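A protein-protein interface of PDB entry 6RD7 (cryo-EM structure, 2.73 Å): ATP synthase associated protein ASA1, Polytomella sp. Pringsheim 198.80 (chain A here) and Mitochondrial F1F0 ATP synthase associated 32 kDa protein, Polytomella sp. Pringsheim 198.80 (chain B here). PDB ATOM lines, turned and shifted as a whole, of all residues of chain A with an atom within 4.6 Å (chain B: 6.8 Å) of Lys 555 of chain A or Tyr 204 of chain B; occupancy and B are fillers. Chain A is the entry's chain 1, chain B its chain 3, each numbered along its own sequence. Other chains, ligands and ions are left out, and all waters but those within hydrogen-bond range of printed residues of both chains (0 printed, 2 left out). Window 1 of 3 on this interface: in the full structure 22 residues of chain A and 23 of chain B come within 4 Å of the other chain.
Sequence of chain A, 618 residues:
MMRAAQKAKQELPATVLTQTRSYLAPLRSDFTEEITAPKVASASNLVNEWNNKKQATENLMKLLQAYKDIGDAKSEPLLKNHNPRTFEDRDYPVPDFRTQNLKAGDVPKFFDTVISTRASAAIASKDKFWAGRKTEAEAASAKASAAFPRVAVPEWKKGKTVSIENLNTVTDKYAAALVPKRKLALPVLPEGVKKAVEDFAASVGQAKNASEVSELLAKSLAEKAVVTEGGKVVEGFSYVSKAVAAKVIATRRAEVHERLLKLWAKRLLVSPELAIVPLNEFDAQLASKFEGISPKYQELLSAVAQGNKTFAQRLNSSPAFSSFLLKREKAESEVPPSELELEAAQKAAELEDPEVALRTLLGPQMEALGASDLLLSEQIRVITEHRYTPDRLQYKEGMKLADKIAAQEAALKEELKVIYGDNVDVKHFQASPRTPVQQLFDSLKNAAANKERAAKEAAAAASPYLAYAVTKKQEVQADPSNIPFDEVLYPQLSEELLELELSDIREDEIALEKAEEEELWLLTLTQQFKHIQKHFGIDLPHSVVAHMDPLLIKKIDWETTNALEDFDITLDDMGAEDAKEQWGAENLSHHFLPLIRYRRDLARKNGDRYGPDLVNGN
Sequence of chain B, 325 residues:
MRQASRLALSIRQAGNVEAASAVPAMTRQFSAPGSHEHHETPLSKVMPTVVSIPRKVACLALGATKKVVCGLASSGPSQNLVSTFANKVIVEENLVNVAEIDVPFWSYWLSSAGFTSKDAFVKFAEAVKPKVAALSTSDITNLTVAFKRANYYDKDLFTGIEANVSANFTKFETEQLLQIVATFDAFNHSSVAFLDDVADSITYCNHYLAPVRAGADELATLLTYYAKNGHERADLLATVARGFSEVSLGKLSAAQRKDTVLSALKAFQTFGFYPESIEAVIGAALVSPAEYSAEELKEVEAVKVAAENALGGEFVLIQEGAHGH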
ATOM      1  N   LEU A 551     -31.694 -21.880  12.600  1.00  0.00           N
ATOM      2  CA  LEU A 551     -30.852 -22.550  13.580  1.00  0.00           C
ATOM      3  C   LEU A 551     -31.168 -22.103  14.995  1.00  0.00           C
ATOM      4  O   LEU A 551     -31.079 -22.910  15.925  1.00  0.00           O
ATOM      5  CB  LEU A 551     -29.373 -22.311  13.281  1.00  0.00           C
ATOM      6  CG  LEU A 551     -28.657 -23.229  12.288  1.00  0.00           C
ATOM      7  CD1 LEU A 551     -28.870 -24.649  12.691  1.00  0.00           C
ATOM      8  CD2 LEU A 551     -29.091 -23.035  10.879  1.00  0.00           C
ATOM      9  N   LEU A 552     -31.551 -20.840  15.177  1.00  0.00           N
ATOM     10  CA  LEU A 552     -31.982 -20.376  16.489  1.00  0.00           C
ATOM     11  C   LEU A 552     -33.279 -21.048  16.906  1.00  0.00           C
ATOM     12  O   LEU A 552     -33.437 -21.444  18.065  1.00  0.00           O
ATOM     13  CB  LEU A 552     -32.142 -18.859  16.476  1.00  0.00           C
ATOM     14  CG  LEU A 552     -32.739 -18.215  17.721  1.00  0.00           C
ATOM     15  CD1 LEU A 552     -31.803 -18.369  18.899  1.00  0.00           C
ATOM     16  CD2 LEU A 552     -33.048 -16.761  17.467  1.00  0.00           C
ATOM     17  N   ILE A 553     -34.200 -21.215  15.958  1.00  0.00           N
ATOM     18  CA  ILE A 553     -35.446 -21.922  16.224  1.00  0.00           C
ATOM     19  C   ILE A 553     -35.175 -23.398  16.488  1.00  0.00           C
ATOM     20  O   ILE A 553     -35.815 -24.010  17.347  1.00  0.00           O
ATOM     21  CB  ILE A 553     -36.421 -21.694  15.054  1.00  0.00           C
ATOM     22  CG1 ILE A 553     -36.786 -20.215  14.970  1.00  0.00           C
ATOM     23  CG2 ILE A 553     -37.682 -22.510  15.192  1.00  0.00           C
ATOM     24  CD1 ILE A 553     -37.291 -19.628  16.261  1.00  0.00           C
ATOM     25  N   LYS A 554     -34.178 -23.968  15.809  1.00  0.00           N
ATOM     26  CA  LYS A 554     -33.774 -25.348  16.067  1.00  0.00           C
ATOM     27  C   LYS A 554     -33.207 -25.518  17.474  1.00  0.00           C
ATOM     28  O   LYS A 554     -33.507 -26.504  18.155  1.00  0.00           O
ATOM     29  CB  LYS A 554     -32.752 -25.777  15.018  1.00  0.00           C
ATOM     30  CG  LYS A 554     -32.226 -27.178  15.165  1.00  0.00           C
ATOM     31  CD  LYS A 554     -30.863 -27.295  14.531  1.00  0.00           C
ATOM     32  CE  LYS A 554     -30.456 -28.736  14.352  1.00  0.00           C
ATOM     33  NZ  LYS A 554     -29.148 -28.832  13.670  1.00  0.00           N
ATOM     34  N   LYS A 555     -32.421 -24.549  17.943  1.00  0.00           N
ATOM     35  CA  LYS A 555     -31.855 -24.640  19.287  1.00  0.00           C
ATOM     36  C   LYS A 555     -32.912 -24.424  20.367  1.00  0.00           C
ATOM     37  O   LYS A 555     -32.900 -25.107  21.401  1.00  0.00           O
ATOM     38  CB  LYS A 555     -30.724 -23.634  19.439  1.00  0.00           C
ATOM     39  CG  LYS A 555     -29.508 -23.967  18.622  1.00  0.00           C
ATOM     40  CD  LYS A 555     -28.628 -22.761  18.466  1.00  0.00           C
ATOM     41  CE  LYS A 555     -27.578 -23.001  17.427  1.00  0.00           C
ATOM     42  NZ  LYS A 555     -26.379 -22.177  17.674  1.00  0.00           N
ATOM     43  N   ILE A 556     -33.839 -23.488  20.144  1.00  0.00           N
ATOM     44  CA  ILE A 556     -34.931 -23.271  21.092  1.00  0.00           C
ATOM     45  C   ILE A 556     -35.854 -24.486  21.125  1.00  0.00           C
ATOM     46  O   ILE A 556     -36.345 -24.890  22.188  1.00  0.00           O
ATOM     47  CB  ILE A 556     -35.682 -21.974  20.735  1.00  0.00           C
ATOM     48  CG1 ILE A 556     -34.784 -20.765  20.958  1.00  0.00           C
ATOM     49  CG2 ILE A 556     -36.918 -21.790  21.575  1.00  0.00           C
ATOM     50  CD1 ILE A 556     -35.266 -19.536  20.261  1.00  0.00           C
ATOM     51  N   ASP A 557     -36.055 -25.123  19.971  1.00  0.00           N
ATOM     52  CA  ASP A 557     -36.854 -26.337  19.918  1.00  0.00           C
ATOM     53  C   ASP A 557     -36.143 -27.497  20.596  1.00  0.00           C
ATOM     54  O   ASP A 557     -36.795 -28.382  21.157  1.00  0.00           O
ATOM     55  CB  ASP A 557     -37.180 -26.683  18.469  1.00  0.00           C
ATOM     56  CG  ASP A 557     -38.287 -25.825  17.899  1.00  0.00           C
ATOM     57  OD1 ASP A 557     -38.856 -25.010  18.650  1.00  0.00           O
ATOM     58  OD2 ASP A 557     -38.585 -25.961  16.697  1.00  0.00           O
ATOM     59  N   TRP A 558     -34.808 -27.521  20.545  1.00  0.00           N
ATOM     60  CA  TRP A 558     -34.065 -28.514  21.315  1.00  0.00           C
ATOM     61  C   TRP A 558     -34.254 -28.299  22.804  1.00  0.00           C
ATOM     62  O   TRP A 558     -34.355 -29.264  23.566  1.00  0.00           O
ATOM     63  CB  TRP A 558     -32.573 -28.470  20.976  1.00  0.00           C
ATOM     64  CG  TRP A 558     -31.784 -29.558  21.668  1.00  0.00           C
ATOM     65  CD1 TRP A 558     -31.505 -30.791  21.175  1.00  0.00           C
ATOM     66  CD2 TRP A 558     -31.193 -29.511  22.978  1.00  0.00           C
ATOM     67  NE1 TRP A 558     -30.781 -31.514  22.084  1.00  0.00           N
ATOM     68  CE2 TRP A 558     -30.577 -30.750  23.200  1.00  0.00           C
ATOM     69  CE3 TRP A 558     -31.132 -28.542  23.984  1.00  0.00           C
ATOM     70  CZ2 TRP A 558     -29.910 -31.047  24.377  1.00  0.00           C
ATOM     71  CZ3 TRP A 558     -30.471 -28.838  25.147  1.00  0.00           C
ATOM     72  CH2 TRP A 558     -29.866 -30.077  25.337  1.00  0.00           C
ATOM     73  N   GLU A 559     -34.252 -27.037  23.238  1.00  0.00           N
ATOM     74  CA  GLU A 559     -34.465 -26.732  24.650  1.00  0.00           C
ATOM     75  C   GLU A 559     -35.853 -27.151  25.110  1.00  0.00           C
ATOM     76  O   GLU A 559     -36.010 -27.694  26.207  1.00  0.00           O
ATOM     77  CB  GLU A 559     -34.266 -25.244  24.902  1.00  0.00           C
ATOM     78  CG  GLU A 559     -32.914 -24.886  25.427  1.00  0.00           C
ATOM     79  CD  GLU A 559     -32.755 -23.402  25.632  1.00  0.00           C
ATOM     80  OE1 GLU A 559     -32.911 -22.938  26.777  1.00  0.00           O
ATOM     81  OE2 GLU A 559     -32.487 -22.691  24.645  1.00  0.00           O
ATOM     82  N   GLU A 586     -24.282 -18.607  22.865  1.00  0.00           N
ATOM     83  CA  GLU A 586     -24.169 -19.891  22.188  1.00  0.00           C
ATOM     84  C   GLU A 586     -25.411 -20.195  21.368  1.00  0.00           C
ATOM     85  O   GLU A 586     -25.350 -20.982  20.419  1.00  0.00           O
ATOM     86  CB  GLU A 586     -23.923 -21.009  23.197  1.00  0.00           C
ATOM     87  CG  GLU A 586     -22.543 -21.024  23.815  1.00  0.00           C
ATOM     88  CD  GLU A 586     -21.492 -21.656  22.937  1.00  0.00           C
ATOM     89  OE1 GLU A 586     -21.849 -22.269  21.910  1.00  0.00           O
ATOM     90  OE2 GLU A 586     -20.300 -21.547  23.284  1.00  0.00           O
ATOM     91  N   ASN A 587     -26.551 -19.599  21.717  1.00  0.00           N
ATOM     92  CA  ASN A 587     -27.731 -19.819  20.891  1.00  0.00           C
ATOM     93  C   ASN A 587     -27.688 -18.980  19.623  1.00  0.00           C
ATOM     94  O   ASN A 587     -28.384 -19.280  18.649  1.00  0.00           O
ATOM     95  CB  ASN A 587     -28.996 -19.527  21.678  1.00  0.00           C
ATOM     96  CG  ASN A 587     -29.376 -20.654  22.602  1.00  0.00           C
ATOM     97  OD1 ASN A 587     -29.129 -21.820  22.312  1.00  0.00           O
ATOM     98  ND2 ASN A 587     -29.995 -20.315  23.717  1.00  0.00           N
ATOM     99  N   SER A 589     -24.627 -18.473  18.160  1.00  0.00           N
ATOM    100  CA  SER A 589     -23.250 -18.700  17.738  1.00  0.00           C
ATOM    101  C   SER A 589     -23.153 -18.980  16.248  1.00  0.00           C
ATOM    102  O   SER A 589     -22.087 -18.806  15.653  1.00  0.00           O
ATOM    103  CB  SER A 589     -22.649 -19.859  18.526  1.00  0.00           C
ATOM    104  OG  SER A 589     -23.293 -21.075  18.201  1.00  0.00           O
ATOM    105  N   HIS A 590     -24.250 -19.414  15.632  1.00  0.00           N
ATOM    106  CA  HIS A 590     -24.263 -19.729  14.214  1.00  0.00           C
ATOM    107  C   HIS A 590     -24.244 -18.494  13.328  1.00  0.00           C
ATOM    108  O   HIS A 590     -24.054 -18.636  12.120  1.00  0.00           O
ATOM    109  CB  HIS A 590     -25.494 -20.564  13.885  1.00  0.00           C
ATOM    110  CG  HIS A 590     -26.781 -19.884  14.220  1.00  0.00           C
ATOM    111  ND1 HIS A 590     -27.290 -19.844  15.498  1.00  0.00           N
ATOM    112  CD2 HIS A 590     -27.655 -19.199  13.447  1.00  0.00           C
ATOM    113  CE1 HIS A 590     -28.423 -19.170  15.497  1.00  0.00           C
ATOM    114  NE2 HIS A 590     -28.668 -18.768  14.265  1.00  0.00           N
ATOM    115  N   LEU A 593     -20.897 -18.294  11.918  1.00  0.00           N
ATOM    116  CA  LEU A 593     -20.477 -19.490  11.189  1.00  0.00           C
ATOM    117  C   LEU A 593     -20.271 -19.300   9.682  1.00  0.00           C
ATOM    118  O   LEU A 593     -19.357 -19.946   9.140  1.00  0.00           O
ATOM    119  CB  LEU A 593     -21.467 -20.622  11.484  1.00  0.00           C
ATOM    120  CG  LEU A 593     -21.392 -21.925  10.693  1.00  0.00           C
ATOM    121  CD1 LEU A 593     -20.122 -22.667  11.020  1.00  0.00           C
ATOM    122  CD2 LEU A 593     -22.587 -22.767  10.992  1.00  0.00           C
ATOM    123  N   ILE A 596     -16.810 -17.859   9.590  1.00  0.00           N
ATOM    124  CA  ILE A 596     -15.817 -18.837  10.023  1.00  0.00           C
ATOM    125  C   ILE A 596     -15.545 -19.851   8.920  1.00  0.00           C
ATOM    126  O   ILE A 596     -14.389 -20.186   8.639  1.00  0.00           O
ATOM    127  CB  ILE A 596     -16.278 -19.514  11.329  1.00  0.00           C
ATOM    128  CG1 ILE A 596     -16.270 -18.513  12.477  1.00  0.00           C
ATOM    129  CG2 ILE A 596     -15.385 -20.665  11.698  1.00  0.00           C
ATOM    130  CD1 ILE A 596     -17.058 -18.973  13.673  1.00  0.00           C
ATOM    131  N   ALA B 199     -17.915 -31.004  12.733  1.00  0.00           N
ATOM    132  CA  ALA B 199     -17.488 -30.118  13.811  1.00  0.00           C
ATOM    133  C   ALA B 199     -18.264 -28.807  13.803  1.00  0.00           C
ATOM    134  O   ALA B 199     -18.655 -28.308  14.864  1.00  0.00           O
ATOM    135  CB  ALA B 199     -15.991 -29.852  13.704  1.00  0.00           C
ATOM    136  N   ASP B 200     -18.527 -28.255  12.613  1.00  0.00           N
ATOM    137  CA  ASP B 200     -19.323 -27.037  12.501  1.00  0.00           C
ATOM    138  C   ASP B 200     -20.757 -27.275  12.941  1.00  0.00           C
ATOM    139  O   ASP B 200     -21.376 -26.407  13.564  1.00  0.00           O
ATOM    140  CB  ASP B 200     -19.304 -26.529  11.061  1.00  0.00           C
ATOM    141  CG  ASP B 200     -18.053 -25.757  10.731  1.00  0.00           C
ATOM    142  OD1 ASP B 200     -17.391 -25.266  11.664  1.00  0.00           O
ATOM    143  OD2 ASP B 200     -17.730 -25.641   9.533  1.00  0.00           O
ATOM    144  N   SER B 201     -21.291 -28.458  12.646  1.00  0.00           N
ATOM    145  CA  SER B 201     -22.669 -28.765  12.990  1.00  0.00           C
ATOM    146  C   SER B 201     -22.838 -28.976  14.486  1.00  0.00           C
ATOM    147  O   SER B 201     -23.844 -28.565  15.070  1.00  0.00           O
ATOM    148  CB  SER B 201     -23.113 -29.999  12.223  1.00  0.00           C
ATOM    149  OG  SER B 201     -24.517 -30.147  12.280  1.00  0.00           O
ATOM    150  N   ILE B 202     -21.867 -29.626  15.122  1.00  0.00           N
ATOM    151  CA  ILE B 202     -21.966 -29.849  16.559  1.00  0.00           C
ATOM    152  C   ILE B 202     -21.684 -28.558  17.319  1.00  0.00           C
ATOM    153  O   ILE B 202     -22.352 -28.250  18.313  1.00  0.00           O
ATOM    154  CB  ILE B 202     -21.030 -30.999  16.974  1.00  0.00           C
ATOM    155  CG1 ILE B 202     -21.530 -32.309  16.370  1.00  0.00           C
ATOM    156  CG2 ILE B 202     -20.945 -31.143  18.481  1.00  0.00           C
ATOM    157  CD1 ILE B 202     -20.701 -33.506  16.724  1.00  0.00           C
ATOM    158  N   THR B 203     -20.746 -27.744  16.832  1.00  0.00           N
ATOM    159  CA  THR B 203     -20.361 -26.551  17.574  1.00  0.00           C
ATOM    160  C   THR B 203     -21.363 -25.419  17.388  1.00  0.00           C
ATOM    161  O   THR B 203     -21.785 -24.795  18.366  1.00  0.00           O
ATOM    162  CB  THR B 203     -18.973 -26.097  17.140  1.00  0.00           C
ATOM    163  OG1 THR B 203     -18.064 -27.191  17.249  1.00  0.00           O
ATOM    164  CG2 THR B 203     -18.489 -24.978  18.029  1.00  0.00           C
ATOM    165  N   TYR B 204     -21.759 -25.142  16.151  1.00  0.00           N
ATOM    166  CA  TYR B 204     -22.529 -23.946  15.848  1.00  0.00           C
ATOM    167  C   TYR B 204     -23.963 -24.212  15.436  1.00  0.00           C
ATOM    168  O   TYR B 204     -24.817 -23.364  15.680  1.00  0.00           O
ATOM    169  CB  TYR B 204     -21.846 -23.140  14.734  1.00  0.00           C
ATOM    170  CG  TYR B 204     -20.398 -22.836  15.013  1.00  0.00           C
ATOM    171  CD1 TYR B 204     -20.040 -21.776  15.827  1.00  0.00           C
ATOM    172  CD2 TYR B 204     -19.390 -23.613  14.466  1.00  0.00           C
ATOM    173  CE1 TYR B 204     -18.720 -21.498  16.090  1.00  0.00           C
ATOM    174  CE2 TYR B 204     -18.070 -23.344  14.723  1.00  0.00           C
ATOM    175  CZ  TYR B 204     -17.741 -22.286  15.534  1.00  0.00           C
ATOM    176  OH  TYR B 204     -16.421 -22.015  15.791  1.00  0.00           O
ATOM    177  N   CYS B 205     -24.257 -25.348  14.817  1.00  0.00           N
ATOM    178  CA  CYS B 205     -25.601 -25.604  14.326  1.00  0.00           C
ATOM    179  C   CYS B 205     -26.476 -26.331  15.328  1.00  0.00           C
ATOM    180  O   CYS B 205     -27.650 -26.569  15.042  1.00  0.00           O
ATOM    181  CB  CYS B 205     -25.556 -26.418  13.035  1.00  0.00           C
ATOM    182  SG  CYS B 205     -24.669 -25.644  11.699  1.00  0.00           S
ATOM    183  N   ASN B 206     -25.946 -26.699  16.482  1.00  0.00           N
ATOM    184  CA  ASN B 206     -26.726 -27.402  17.478  1.00  0.00           C
ATOM    185  C   ASN B 206     -26.617 -26.676  18.804  1.00  0.00           C
ATOM    186  O   ASN B 206     -25.828 -25.743  18.958  1.00  0.00           O
ATOM    187  CB  ASN B 206     -26.269 -28.846  17.619  1.00  0.00           C
ATOM    188  CG  ASN B 206     -26.886 -29.736  16.582  1.00  0.00           C
ATOM    189  OD1 ASN B 206     -26.209 -30.232  15.687  1.00  0.00           O
ATOM    190  ND2 ASN B 206     -28.187 -29.933  16.686  1.00  0.00           N
ATOM    191  N   HIS B 207     -27.436 -27.111  19.756  1.00  0.00           N
ATOM    192  CA  HIS B 207     -27.423 -26.502  21.074  1.00  0.00           C
ATOM    193  C   HIS B 207     -26.125 -26.836  21.789  1.00  0.00           C
ATOM    194  O   HIS B 207     -25.558 -27.914  21.612  1.00  0.00           O
ATOM    195  CB  HIS B 207     -28.617 -26.978  21.893  1.00  0.00           C
ATOM    196  CG  HIS B 207     -28.995 -26.042  22.995  1.00  0.00           C
ATOM    197  ND1 HIS B 207     -28.440 -26.111  24.251  1.00  0.00           N
ATOM    198  CD2 HIS B 207     -29.864 -25.007  23.025  1.00  0.00           C
ATOM    199  CE1 HIS B 207     -28.952 -25.161  25.010  1.00  0.00           C
ATOM    200  NE2 HIS B 207     -29.816 -24.475  24.289  1.00  0.00           N
ATOM    201  N   TYR B 208     -25.642 -25.889  22.588  1.00  0.00           N
ATOM    202  CA  TYR B 208     -24.357 -26.076  23.245  1.00  0.00           C
ATOM    203  C   TYR B 208     -24.457 -27.036  24.421  1.00  0.00           C
ATOM    204  O   TYR B 208     -23.433 -27.523  24.908  1.00  0.00           O
ATOM    205  CB  TYR B 208     -23.791 -24.724  23.674  1.00  0.00           C
ATOM    206  CG  TYR B 208     -24.397 -24.123  24.917  1.00  0.00           C
ATOM    207  CD1 TYR B 208     -25.704 -23.654  24.929  1.00  0.00           C
ATOM    208  CD2 TYR B 208     -23.649 -23.993  26.071  1.00  0.00           C
ATOM    209  CE1 TYR B 208     -26.246 -23.098  26.061  1.00  0.00           C
ATOM    210  CE2 TYR B 208     -24.181 -23.437  27.197  1.00  0.00           C
ATOM    211  CZ  TYR B 208     -25.475 -22.993  27.192  1.00  0.00           C
ATOM    212  OH  TYR B 208     -25.994 -22.442  28.333  1.00  0.00           O
ATOM    213  N   ARG B 233     -10.065 -29.260  15.969  1.00  0.00           N
ATOM    214  CA  ARG B 233     -10.948 -28.106  16.055  1.00  0.00           C
ATOM    215  C   ARG B 233     -11.132 -27.774  17.526  1.00  0.00           C
ATOM    216  O   ARG B 233     -11.736 -28.556  18.266  1.00  0.00           O
ATOM    217  CB  ARG B 233     -12.290 -28.398  15.388  1.00  0.00           C
ATOM    218  CG  ARG B 233     -12.196 -28.648  13.901  1.00  0.00           C
ATOM    219  CD  ARG B 233     -12.353 -27.358  13.137  1.00  0.00           C
ATOM    220  NE  ARG B 233     -13.506 -26.609  13.614  1.00  0.00           N
ATOM    221  CZ  ARG B 233     -14.674 -26.563  12.988  1.00  0.00           C
ATOM    222  NH1 ARG B 233     -14.841 -27.219  11.853  1.00  0.00           N
ATOM    223  NH2 ARG B 233     -15.670 -25.856  13.497  1.00  0.00           N
ATOM    224  N   ASP B 235     -12.866 -25.397  18.953  1.00  0.00           N
ATOM    225  CA  ASP B 235     -14.241 -25.077  19.317  1.00  0.00           C
ATOM    226  C   ASP B 235     -15.065 -26.341  19.527  1.00  0.00           C
ATOM    227  O   ASP B 235     -15.828 -26.442  20.499  1.00  0.00           O
ATOM    228  CB  ASP B 235     -14.861 -24.191  18.239  1.00  0.00           C
ATOM    229  CG  ASP B 235     -14.527 -24.659  16.837  1.00  0.00           C
ATOM    230  OD1 ASP B 235     -13.837 -25.685  16.702  1.00  0.00           O
ATOM    231  OD2 ASP B 235     -14.949 -23.999  15.867  1.00  0.00           O
ATOM    232  N   LEU B 236     -14.905 -27.322  18.634  1.00  0.00           N
ATOM    233  CA  LEU B 236     -15.535 -28.622  18.827  1.00  0.00           C
ATOM    234  C   LEU B 236     -14.984 -29.317  20.060  1.00  0.00           C
ATOM    235  O   LEU B 236     -15.723 -29.998  20.774  1.00  0.00           O
ATOM    236  CB  LEU B 236     -15.338 -29.495  17.588  1.00  0.00           C
ATOM    237  CG  LEU B 236     -15.798 -30.949  17.704  1.00  0.00           C
ATOM    238  CD1 LEU B 236     -17.282 -31.066  17.458  1.00  0.00           C
ATOM    239  CD2 LEU B 236     -15.030 -31.847  16.784  1.00  0.00           C
ATOM    240  N   THR B 239     -16.783 -27.796  22.986  1.00  0.00           N
ATOM    241  CA  THR B 239     -18.184 -28.218  22.993  1.00  0.00           C
ATOM    242  C   THR B 239     -18.337 -29.659  23.473  1.00  0.00           C
ATOM    243  O   THR B 239     -19.155 -29.947  24.352  1.00  0.00           O
ATOM    244  CB  THR B 239     -18.778 -28.043  21.591  1.00  0.00           C
ATOM    245  OG1 THR B 239     -18.986 -26.650  21.334  1.00  0.00           O
ATOM    246  CG2 THR B 239     -20.102 -28.760  21.455  1.00  0.00           C
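The backbone carbonyl oxygen (O) of Asp 200 of chain B is in hydrogen-bond range of the backbone NH (N) of Cys 205 of chain B, 3.3 Å away.
O of Asn 587 of chain A sits close to ND1 of His 590 of chain A.
The side-chain amino group (NZ) of Lys 555 of chain A lies within hydrogen-bond range of the backbone carbonyl oxygen (O) of Glu 586 of chain A, 3.2 Å away.
The side-chain amino group (NZ) of Lys 555 of chain A sits at hydrogen-bond distance from a ring nitrogen (ND1) of His 590 of chain A (3.3 Å).
The backbone carbonyl oxygen of Ser 201 of chain B sits close to the side-chain amide oxygen of Asn 206 of chain B (3.0 Å).
The side-chain hydroxyl (OH) of Tyr 204 of chain B is in hydrogen-bond range of the side-chain carboxylate (OD2) of Asp 235 of chain B.
Leu 551 of chain A touches Cys 205 of chain B (CD1 to O, 3.3 Å).
His 207 of chain B touches Lys 555 of chain A.
Trp 558 of chain A touches His 207 of chain B.
CG of Tyr 208 of chain B touches CB of Glu 586 of chain A (3.6 Å).
Ser 589 of chain A touches Tyr 204 of chain B (O to CD1, 3.6 Å).
His 590 of chain A touches Tyr 204 of chain B (CB to O, 3.4 Å).
Leu 593 of chain A touches Asp 200 of chain B.
CD1 of Leu 593 of chain A touches CD2 of Tyr 204 of chain B (3.6 Å).
Cys 205 of chain B touches Leu 593 of chain A (SG to CD2, 3.6 Å).
Ile 596 of chain A touches Tyr 204 of chain B.
Printed residues of chain A that touch a printed residue of chain B: Leu 551, Lys 554, Lys 555, Trp 558, Glu 559, Glu 586, Asn 587, Ser 589, His 590, Leu 593 and Ile 596.
Hydrophobic or aromatic side chains of chain A within 4 Å of the printed part of chain B: Leu 551, Trp 558, His 590, Leu 593 and Ile 596.
Of the 14 printed residues of chain B, 6 touch a printed residue of chain A.
Hydrophobic or aromatic side chains of chain B within 4 Å of the printed part of chain A: Tyr 204, His 207 and Tyr 208.
ND2 of Asn 206 of chain B sits close to NZ of Lys 554 of chain A.
The side-chain amino group (NZ) of Lys 555 of chain A is in hydrogen-bond range of the backbone carbonyl oxygen (O) of Tyr 204 of chain B, 2.8 Å away.
The side-chain amino group (NZ) of Lys 554 of chain A is in hydrogen-bond range of the backbone carbonyl oxygen (O) of Cys 205 of chain B (3.0 Å).
A ring nitrogen (NE2) of His 207 of chain B lies close to the side-chain amide oxygen (OD1) of Asn 587 of chain A, 3.4 Å away.
A ring nitrogen (NE2) of His 207 of chain B sits at hydrogen-bond distance from the side-chain carboxylate (OE2) of Glu 559 of chain A (3.2 Å).
Lys 555 of chain A touches just these residues of chain B: Tyr 204, Asn 206 and His 207.
Of chain A, only Lys 555 (2.8 Å), Ser 589 (3.6 Å), His 590 (3.4 Å), Leu 593 (3.6 Å) and Ile 596 (3.8 Å) come within 4 Å of Tyr 204 of chain B.
Printed residues of chain B within 4 Å of Ile 596 of chain A: Tyr 204.
Of the printed residues of chain B, Leu 593 of chain A touches Asp 200 (3.7 Å), Tyr 204 (3.6 Å) and Cys 205 (3.6 Å).
Of the printed residues of chain A, His 207 of chain B touches Lys 555 (3.4 Å), Trp 558 (3.4 Å), Glu 559 (3.2 Å) and Asn 587 (3.3 Å).
Of the printed residues of chain B, Glu 559 of chain A touches His 207.
The nearest residue of chain B that does not touch Lys 555 of chain A is Cys 205 of chain B (4.1 Å).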
